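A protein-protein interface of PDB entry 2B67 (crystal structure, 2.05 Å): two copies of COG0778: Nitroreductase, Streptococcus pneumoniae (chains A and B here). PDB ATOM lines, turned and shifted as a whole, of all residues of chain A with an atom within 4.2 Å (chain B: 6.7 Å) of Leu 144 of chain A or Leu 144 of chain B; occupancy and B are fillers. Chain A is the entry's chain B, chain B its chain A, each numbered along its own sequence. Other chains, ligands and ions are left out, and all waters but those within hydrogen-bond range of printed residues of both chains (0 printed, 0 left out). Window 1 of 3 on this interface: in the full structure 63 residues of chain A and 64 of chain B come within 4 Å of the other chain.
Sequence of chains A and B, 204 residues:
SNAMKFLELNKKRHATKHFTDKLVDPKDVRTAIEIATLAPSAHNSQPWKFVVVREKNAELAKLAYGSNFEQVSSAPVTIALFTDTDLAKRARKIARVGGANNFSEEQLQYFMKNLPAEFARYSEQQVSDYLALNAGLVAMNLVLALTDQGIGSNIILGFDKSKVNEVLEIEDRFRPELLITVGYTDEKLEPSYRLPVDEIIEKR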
ATOM      1  N   PHE A   6      30.466 -31.124   1.834  1.00  0.00           N
ATOM      2  CA  PHE A   6      29.489 -30.052   1.712  1.00  0.00           C
ATOM      3  C   PHE A   6      29.941 -28.806   2.450  1.00  0.00           C
ATOM      4  O   PHE A   6      29.733 -27.694   1.965  1.00  0.00           O
ATOM      5  CB  PHE A   6      28.108 -30.519   2.196  1.00  0.00           C
ATOM      6  CG  PHE A   6      27.005 -29.541   1.922  1.00  0.00           C
ATOM      7  CD1 PHE A   6      26.764 -29.087   0.634  1.00  0.00           C
ATOM      8  CD2 PHE A   6      26.198 -29.084   2.950  1.00  0.00           C
ATOM      9  CE1 PHE A   6      25.713 -28.170   0.389  1.00  0.00           C
ATOM     10  CE2 PHE A   6      25.156 -28.185   2.720  1.00  0.00           C
ATOM     11  CZ  PHE A   6      24.907 -27.731   1.445  1.00  0.00           C
ATOM     12  N   LEU A   9      32.335 -27.126  -0.044  1.00  0.00           N
ATOM     13  CA  LEU A   9      31.558 -26.445  -1.078  1.00  0.00           C
ATOM     14  C   LEU A   9      31.016 -25.096  -0.546  1.00  0.00           C
ATOM     15  O   LEU A   9      31.140 -24.060  -1.187  1.00  0.00           O
ATOM     16  CB  LEU A   9      30.394 -27.345  -1.549  1.00  0.00           C
ATOM     17  CG  LEU A   9      29.707 -27.251  -2.920  1.00  0.00           C
ATOM     18  CD1 LEU A   9      28.252 -27.696  -2.860  1.00  0.00           C
ATOM     19  CD2 LEU A   9      29.759 -25.903  -3.468  1.00  0.00           C
ATOM     20  N   MET A 140      19.043 -21.223  -3.456  1.00  0.00           N
ATOM     21  CA  MET A 140      20.172 -21.755  -2.695  1.00  0.00           C
ATOM     22  C   MET A 140      20.833 -22.914  -3.451  1.00  0.00           C
ATOM     23  O   MET A 140      22.070 -22.973  -3.555  1.00  0.00           O
ATOM     24  CB  MET A 140      19.723 -22.241  -1.302  1.00  0.00           C
ATOM     25  CG  MET A 140      20.842 -22.870  -0.503  1.00  0.00           C
ATOM     26  SD  MET A 140      21.923 -21.458   0.337  1.00  0.00           S
ATOM     27  CE  MET A 140      23.599 -21.612  -0.479  1.00  0.00           C
ATOM     28  N   ASN A 141      19.999 -23.821  -3.977  1.00  0.00           N
ATOM     29  CA  ASN A 141      20.477 -25.044  -4.679  1.00  0.00           C
ATOM     30  C   ASN A 141      21.206 -24.673  -5.970  1.00  0.00           C
ATOM     31  O   ASN A 141      22.227 -25.287  -6.292  1.00  0.00           O
ATOM     32  CB  ASN A 141      19.327 -26.058  -4.945  1.00  0.00           C
ATOM     33  CG  ASN A 141      19.761 -27.539  -4.752  1.00  0.00           C
ATOM     34  OD1 ASN A 141      20.694 -27.814  -4.030  1.00  0.00           O
ATOM     35  ND2 ASN A 141      19.043 -28.483  -5.377  1.00  0.00           N
ATOM     36  N   LEU A 142      20.694 -23.661  -6.677  1.00  0.00           N
ATOM     37  CA  LEU A 142      21.308 -23.169  -7.928  1.00  0.00           C
ATOM     38  C   LEU A 142      22.717 -22.624  -7.677  1.00  0.00           C
ATOM     39  O   LEU A 142      23.674 -22.976  -8.353  1.00  0.00           O
ATOM     40  CB  LEU A 142      20.435 -22.062  -8.569  1.00  0.00           C
ATOM     41  CG  LEU A 142      20.964 -21.407  -9.869  1.00  0.00           C
ATOM     42  CD1 LEU A 142      21.434 -22.468 -10.899  1.00  0.00           C
ATOM     43  CD2 LEU A 142      19.957 -20.458 -10.492  1.00  0.00           C
ATOM     44  N   VAL A 143      22.808 -21.772  -6.664  1.00  0.00           N
ATOM     45  CA  VAL A 143      24.030 -21.115  -6.265  1.00  0.00           C
ATOM     46  C   VAL A 143      25.125 -22.117  -5.850  1.00  0.00           C
ATOM     47  O   VAL A 143      26.308 -21.968  -6.220  1.00  0.00           O
ATOM     48  CB  VAL A 143      23.629 -20.064  -5.160  1.00  0.00           C
ATOM     49  CG1 VAL A 143      24.365 -20.222  -3.918  1.00  0.00           C
ATOM     50  CG2 VAL A 143      23.635 -18.645  -5.696  1.00  0.00           C
ATOM     51  N   LEU A 144      24.734 -23.163  -5.126  1.00  0.00           N
ATOM     52  CA  LEU A 144      25.660 -24.258  -4.816  1.00  0.00           C
ATOM     53  C   LEU A 144      26.067 -25.071  -6.043  1.00  0.00           C
ATOM     54  O   LEU A 144      27.252 -25.420  -6.186  1.00  0.00           O
ATOM     55  CB  LEU A 144      25.078 -25.196  -3.766  1.00  0.00           C
ATOM     56  CG  LEU A 144      24.882 -24.561  -2.370  1.00  0.00           C
ATOM     57  CD1 LEU A 144      24.007 -25.462  -1.472  1.00  0.00           C
ATOM     58  CD2 LEU A 144      26.231 -24.255  -1.708  1.00  0.00           C
ATOM     59  N   ALA A 145      25.082 -25.416  -6.878  1.00  0.00           N
ATOM     60  CA  ALA A 145      25.327 -26.075  -8.179  1.00  0.00           C
ATOM     61  C   ALA A 145      26.368 -25.318  -9.018  1.00  0.00           C
ATOM     62  O   ALA A 145      27.353 -25.910  -9.480  1.00  0.00           O
ATOM     63  CB  ALA A 145      24.006 -26.265  -8.960  1.00  0.00           C
ATOM     64  N   LEU A 146      26.189 -24.016  -9.158  1.00  0.00           N
ATOM     65  CA  LEU A 146      27.186 -23.174  -9.836  1.00  0.00           C
ATOM     66  C   LEU A 146      28.553 -23.259  -9.157  1.00  0.00           C
ATOM     67  O   LEU A 146      29.580 -23.504  -9.816  1.00  0.00           O
ATOM     68  CB  LEU A 146      26.706 -21.711  -9.904  1.00  0.00           C
ATOM     69  CG  LEU A 146      25.443 -21.459 -10.746  1.00  0.00           C
ATOM     70  CD1 LEU A 146      24.858 -20.064 -10.500  1.00  0.00           C
ATOM     71  CD2 LEU A 146      25.761 -21.659 -12.235  1.00  0.00           C
ATOM     72  N   THR A 147      28.564 -23.093  -7.830  1.00  0.00           N
ATOM     73  CA  THR A 147      29.804 -23.169  -7.072  1.00  0.00           C
ATOM     74  C   THR A 147      30.557 -24.482  -7.332  1.00  0.00           C
ATOM     75  O   THR A 147      31.810 -24.508  -7.429  1.00  0.00           O
ATOM     76  CB  THR A 147      29.581 -22.973  -5.568  1.00  0.00           C
ATOM     77  OG1 THR A 147      28.876 -21.743  -5.330  1.00  0.00           O
ATOM     78  CG2 THR A 147      30.923 -22.918  -4.820  1.00  0.00           C
ATOM     79  N   ASP A 148      29.799 -25.569  -7.413  1.00  0.00           N
ATOM     80  CA  ASP A 148      30.379 -26.887  -7.544  1.00  0.00           C
ATOM     81  C   ASP A 148      31.061 -27.005  -8.920  1.00  0.00           C
ATOM     82  O   ASP A 148      31.970 -27.800  -9.073  1.00  0.00           O
ATOM     83  CB  ASP A 148      29.279 -27.952  -7.401  1.00  0.00           C
ATOM     84  CG  ASP A 148      29.828 -29.380  -7.378  1.00  0.00           C
ATOM     85  OD1 ASP A 148      29.348 -30.219  -8.161  1.00  0.00           O
ATOM     86  OD2 ASP A 148      30.715 -29.674  -6.560  1.00  0.00           O
ATOM     87  N   PHE B   6      28.141 -32.659  -6.006  1.00  0.00           N
ATOM     88  CA  PHE B   6      26.947 -31.984  -5.491  1.00  0.00           C
ATOM     89  C   PHE B   6      25.669 -32.634  -6.042  1.00  0.00           C
ATOM     90  O   PHE B   6      24.685 -32.756  -5.334  1.00  0.00           O
ATOM     91  CB  PHE B   6      27.005 -30.469  -5.745  1.00  0.00           C
ATOM     92  CG  PHE B   6      25.827 -29.712  -5.207  1.00  0.00           C
ATOM     93  CD1 PHE B   6      25.589 -29.649  -3.834  1.00  0.00           C
ATOM     94  CD2 PHE B   6      24.964 -29.054  -6.064  1.00  0.00           C
ATOM     95  CE1 PHE B   6      24.503 -28.940  -3.342  1.00  0.00           C
ATOM     96  CE2 PHE B   6      23.879 -28.345  -5.592  1.00  0.00           C
ATOM     97  CZ  PHE B   6      23.626 -28.301  -4.224  1.00  0.00           C
ATOM     98  N   LEU B   9      25.010 -35.544  -3.786  1.00  0.00           N
ATOM     99  CA  LEU B   9      24.330 -35.107  -2.557  1.00  0.00           C
ATOM    100  C   LEU B   9      22.829 -34.956  -2.791  1.00  0.00           C
ATOM    101  O   LEU B   9      22.012 -35.446  -2.022  1.00  0.00           O
ATOM    102  CB  LEU B   9      24.888 -33.759  -2.086  1.00  0.00           C
ATOM    103  CG  LEU B   9      25.239 -33.532  -0.611  1.00  0.00           C
ATOM    104  CD1 LEU B   9      25.207 -32.058  -0.226  1.00  0.00           C
ATOM    105  CD2 LEU B   9      24.393 -34.358   0.332  1.00  0.00           C
ATOM    106  N   ASN B  10      22.478 -34.254  -3.859  1.00  0.00           N
ATOM    107  CA  ASN B  10      21.083 -33.966  -4.186  1.00  0.00           C
ATOM    108  C   ASN B  10      20.265 -35.206  -4.461  1.00  0.00           C
ATOM    109  O   ASN B  10      19.117 -35.292  -4.068  1.00  0.00           O
ATOM    110  CB  ASN B  10      20.995 -33.007  -5.368  1.00  0.00           C
ATOM    111  CG  ASN B  10      20.817 -31.564  -4.921  1.00  0.00           C
ATOM    112  OD1 ASN B  10      19.696 -31.092  -4.674  1.00  0.00           O
ATOM    113  ND2 ASN B  10      21.917 -30.875  -4.783  1.00  0.00           N
ATOM    114  N   ARG B  13      19.077 -36.703  -1.166  1.00  0.00           N
ATOM    115  CA  ARG B  13      18.108 -36.004  -0.327  1.00  0.00           C
ATOM    116  C   ARG B  13      16.705 -36.464  -0.746  1.00  0.00           C
ATOM    117  O   ARG B  13      16.355 -36.398  -1.910  1.00  0.00           O
ATOM    118  CB  ARG B  13      18.242 -34.481  -0.445  1.00  0.00           C
ATOM    119  CG  ARG B  13      17.361 -33.716   0.551  1.00  0.00           C
ATOM    120  CD  ARG B  13      16.657 -32.512  -0.037  1.00  0.00           C
ATOM    121  NE  ARG B  13      16.150 -32.698  -1.402  1.00  0.00           N
ATOM    122  CZ  ARG B  13      14.934 -33.122  -1.732  1.00  0.00           C
ATOM    123  NH1 ARG B  13      14.044 -33.451  -0.809  1.00  0.00           N
ATOM    124  NH2 ARG B  13      14.597 -33.211  -3.015  1.00  0.00           N
ATOM    125  N   ALA B 139      16.821 -23.046   4.733  1.00  0.00           N
ATOM    126  CA  ALA B 139      16.212 -24.337   4.924  1.00  0.00           C
ATOM    127  C   ALA B 139      16.842 -25.367   3.978  1.00  0.00           C
ATOM    128  O   ALA B 139      17.140 -26.478   4.387  1.00  0.00           O
ATOM    129  CB  ALA B 139      14.728 -24.268   4.710  1.00  0.00           C
ATOM    130  N   MET B 140      17.020 -24.985   2.714  1.00  0.00           N
ATOM    131  CA  MET B 140      17.724 -25.804   1.701  1.00  0.00           C
ATOM    132  C   MET B 140      19.154 -26.230   2.123  1.00  0.00           C
ATOM    133  O   MET B 140      19.528 -27.408   2.014  1.00  0.00           O
ATOM    134  CB  MET B 140      17.813 -25.045   0.378  1.00  0.00           C
ATOM    135  CG  MET B 140      18.507 -25.830  -0.757  1.00  0.00           C
ATOM    136  SD  MET B 140      17.224 -27.095  -1.532  1.00  0.00           S
ATOM    137  CE  MET B 140      17.694 -28.759  -0.646  1.00  0.00           C
ATOM    138  N   ASN B 141      19.916 -25.270   2.631  1.00  0.00           N
ATOM    139  CA  ASN B 141      21.311 -25.521   3.031  1.00  0.00           C
ATOM    140  C   ASN B 141      21.316 -26.521   4.209  1.00  0.00           C
ATOM    141  O   ASN B 141      22.130 -27.448   4.245  1.00  0.00           O
ATOM    142  CB  ASN B 141      22.016 -24.197   3.393  1.00  0.00           C
ATOM    143  CG  ASN B 141      23.498 -24.177   2.976  1.00  0.00           C
ATOM    144  OD1 ASN B 141      23.917 -24.907   2.078  1.00  0.00           O
ATOM    145  ND2 ASN B 141      24.282 -23.328   3.618  1.00  0.00           N
ATOM    146  N   LEU B 142      20.340 -26.356   5.105  1.00  0.00           N
ATOM    147  CA  LEU B 142      20.182 -27.234   6.291  1.00  0.00           C
ATOM    148  C   LEU B 142      19.866 -28.691   5.931  1.00  0.00           C
ATOM    149  O   LEU B 142      20.489 -29.616   6.470  1.00  0.00           O
ATOM    150  CB  LEU B 142      19.086 -26.698   7.207  1.00  0.00           C
ATOM    151  CG  LEU B 142      18.694 -27.598   8.391  1.00  0.00           C
ATOM    152  CD1 LEU B 142      19.929 -27.866   9.270  1.00  0.00           C
ATOM    153  CD2 LEU B 142      17.534 -26.967   9.195  1.00  0.00           C
ATOM    154  N   VAL B 143      18.895 -28.899   5.040  1.00  0.00           N
ATOM    155  CA  VAL B 143      18.566 -30.274   4.669  1.00  0.00           C
ATOM    156  C   VAL B 143      19.715 -30.972   3.923  1.00  0.00           C
ATOM    157  O   VAL B 143      19.930 -32.205   4.075  1.00  0.00           O
ATOM    158  CB  VAL B 143      17.196 -30.430   3.950  1.00  0.00           C
ATOM    159  CG1 VAL B 143      16.048 -29.953   4.841  1.00  0.00           C
ATOM    160  CG2 VAL B 143      17.176 -29.759   2.621  1.00  0.00           C
ATOM    161  N   LEU B 144      20.448 -30.189   3.123  1.00  0.00           N
ATOM    162  CA  LEU B 144      21.631 -30.710   2.428  1.00  0.00           C
ATOM    163  C   LEU B 144      22.739 -31.055   3.401  1.00  0.00           C
ATOM    164  O   LEU B 144      23.369 -32.125   3.277  1.00  0.00           O
ATOM    165  CB  LEU B 144      22.148 -29.730   1.358  1.00  0.00           C
ATOM    166  CG  LEU B 144      21.228 -29.598   0.141  1.00  0.00           C
ATOM    167  CD1 LEU B 144      21.654 -28.342  -0.667  1.00  0.00           C
ATOM    168  CD2 LEU B 144      21.291 -30.858  -0.692  1.00  0.00           C
ATOM    169  N   ALA B 145      22.953 -30.176   4.384  1.00  0.00           N
ATOM    170  CA  ALA B 145      23.946 -30.452   5.417  1.00  0.00           C
ATOM    171  C   ALA B 145      23.607 -31.730   6.213  1.00  0.00           C
ATOM    172  O   ALA B 145      24.485 -32.523   6.513  1.00  0.00           O
ATOM    173  CB  ALA B 145      24.173 -29.216   6.348  1.00  0.00           C
ATOM    174  N   LEU B 146      22.335 -31.931   6.538  1.00  0.00           N
ATOM    175  CA  LEU B 146      21.863 -33.153   7.218  1.00  0.00           C
ATOM    176  C   LEU B 146      22.107 -34.389   6.359  1.00  0.00           C
ATOM    177  O   LEU B 146      22.637 -35.433   6.841  1.00  0.00           O
ATOM    178  CB  LEU B 146      20.359 -33.029   7.540  1.00  0.00           C
ATOM    179  CG  LEU B 146      20.037 -32.057   8.701  1.00  0.00           C
ATOM    180  CD1 LEU B 146      18.528 -31.771   8.866  1.00  0.00           C
ATOM    181  CD2 LEU B 146      20.657 -32.529  10.020  1.00  0.00           C
ATOM    182  N   THR B 147      21.723 -34.258   5.085  1.00  0.00           N
ATOM    183  CA  THR B 147      21.890 -35.299   4.083  1.00  0.00           C
ATOM    184  C   THR B 147      23.349 -35.682   3.985  1.00  0.00           C
ATOM    185  O   THR B 147      23.669 -36.863   3.991  1.00  0.00           O
ATOM    186  CB  THR B 147      21.389 -34.855   2.690  1.00  0.00           C
ATOM    187  OG1 THR B 147      19.989 -34.539   2.751  1.00  0.00           O
ATOM    188  CG2 THR B 147      21.625 -35.968   1.641  1.00  0.00           C
ATOM    189  N   ASP B 148      24.226 -34.684   3.869  1.00  0.00           N
ATOM    190  CA  ASP B 148      25.671 -34.934   3.876  1.00  0.00           C
ATOM    191  C   ASP B 148      26.192 -35.745   5.071  1.00  0.00           C
ATOM    192  O   ASP B 148      27.215 -36.403   4.973  1.00  0.00           O
ATOM    193  CB  ASP B 148      26.457 -33.622   3.820  1.00  0.00           C
ATOM    194  CG  ASP B 148      27.914 -33.841   3.421  1.00  0.00           C
ATOM    195  OD1 ASP B 148      28.812 -33.480   4.213  1.00  0.00           O
ATOM    196  OD2 ASP B 148      28.142 -34.402   2.325  1.00  0.00           O
ATOM    197  N   GLN B 149      25.513 -35.654   6.209  1.00  0.00           N
ATOM    198  CA  GLN B 149      25.895 -36.439   7.348  1.00  0.00           C
ATOM    199  C   GLN B 149      25.150 -37.749   7.419  1.00  0.00           C
ATOM    200  O   GLN B 149      25.279 -38.448   8.400  1.00  0.00           O
ATOM    201  CB  GLN B 149      25.627 -35.696   8.634  1.00  0.00           C
ATOM    202  CG  GLN B 149      26.317 -34.377   8.784  1.00  0.00           C
ATOM    203  CD  GLN B 149      26.260 -33.917  10.234  1.00  0.00           C
ATOM    204  OE1 GLN B 149      26.367 -34.748  11.140  1.00  0.00           O
ATOM    205  NE2 GLN B 149      26.113 -32.606  10.464  1.00  0.00           N
ATOM    206  N   ILE B 151      21.818 -38.085   7.412  1.00  0.00           N
ATOM    207  CA  ILE B 151      20.584 -37.879   8.205  1.00  0.00           C
ATOM    208  C   ILE B 151      19.437 -37.411   7.287  1.00  0.00           C
ATOM    209  O   ILE B 151      19.613 -36.472   6.482  1.00  0.00           O
ATOM    210  CB  ILE B 151      20.825 -36.920   9.402  1.00  0.00           C
ATOM    211  CG1 ILE B 151      21.976 -37.465  10.289  1.00  0.00           C
ATOM    212  CG2 ILE B 151      19.528 -36.731  10.281  1.00  0.00           C
ATOM    213  CD1 ILE B 151      22.530 -36.462  11.315  1.00  0.00           C
ATOM    214  N   SER B 153      15.396 -36.052   6.509  1.00  0.00           N
ATOM    215  CA  SER B 153      14.626 -34.885   6.959  1.00  0.00           C
ATOM    216  C   SER B 153      13.438 -34.707   6.053  1.00  0.00           C
ATOM    217  O   SER B 153      13.414 -35.245   4.952  1.00  0.00           O
ATOM    218  CB  SER B 153      15.471 -33.594   6.907  1.00  0.00           C
ATOM    219  OG  SER B 153      16.080 -33.406   5.625  1.00  0.00           O
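The backbone NH of Phe 6 of chain B sits close to the side-chain carboxylate of Asp 148 of chain A (3.5 Å).
The side-chain amide nitrogen (ND2) of Asn 141 of chain A lies within hydrogen-bond range of the side-chain amide oxygen (OD1) of Asn 10 of chain B (2.8 Å).
Among the printed residues, merely in contact across the chains: Asn 141 of chain A with Phe 6 of chain B, Phe 6 of chain A with Asn 141 of chain B, Phe 6 of chain A with Ala 145 of chain B, Phe 6 of chain A with Leu 144 of chain B, Ala 145 of chain A with Phe 6 of chain B, Leu 9 of chain A with Phe 6 of chain B, Leu 144 of chain A with Phe 6 of chain B, Phe 6 of chain A with Leu 9 of chain B, Asn 141 of chain A with Leu 144 of chain B, Phe 6 of chain A with Asp 148 of chain B, Leu 144 of chain A with Asn 141 of chain B, Met 140 of chain A with Met 140 of chain B, Leu 144 of chain A with Leu 144 of chain B and Phe 6 of chain A with Phe 6 of chain B.
Phe 6 of chain A touches Asn 141 of chain B, and with the chains exchanged Asn 141 of chain A touches Phe 6 of chain B.
Met 140 of chain B touches its own counterpart, Met 140 of chain A.
Asn 141 of chain A touches Leu 144 of chain B, and with the chains exchanged Leu 144 of chain A touches Asn 141 of chain B.
Leu 144 of chain B touches its own counterpart, Leu 144 of chain A.
Positions printed for both chains: 6, 9, 140, 141, 142, 143, 144, 145, 146, 147 and 148.
Of chain B, only Phe 6 (3.5 Å), Asn 141 (3.6 Å) and Leu 144 (3.8 Å) come within 4 Å of Leu 144 of chain A.
Of the printed residues of chain A, Leu 9 of chain B touches Phe 6.
Printed residues of chain B within 4 Å of Ala 145 of chain A: Phe 6 (3.4 Å).
Printed residues of chain A within 4 Å of Ala 145 of chain B: Phe 6 (3.4 Å).
Leu 146 of chain A touches none of the printed residues of chain B.
The nearest printed residue of chain A that does not touch Leu 144 of chain B is Met 140 of chain A (5.5 Å).
The nearest printed residue of chain A that does not touch Asn 10 of chain B is Ala 145 of chain A (6.6 Å).
Hydrophobic or aromatic side chains of chain A within 4 Å of the printed part of chain B: Phe 6, Leu 9, Met 140, Leu 144 and Ala 145.
Printed residues of chain B that touch a printed residue of chain A: Phe 6, Leu 9, Asn 10, Met 140, Asn 141, Leu 144, Ala 145 and Asp 148.
Hydrophobic or aromatic side chains of chain B that line the printed part of chain A: Phe 6, Leu 9, Met 140, Leu 144 and Ala 145.
Among the printed residues, no Asp or Glu carboxylate lies within 4 Å of a Lys or Arg side-chain nitrogen of the other chain.
O of Phe 6 of chain B lies close to ND2 of Asn 10 of chain B (3.4 Å).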
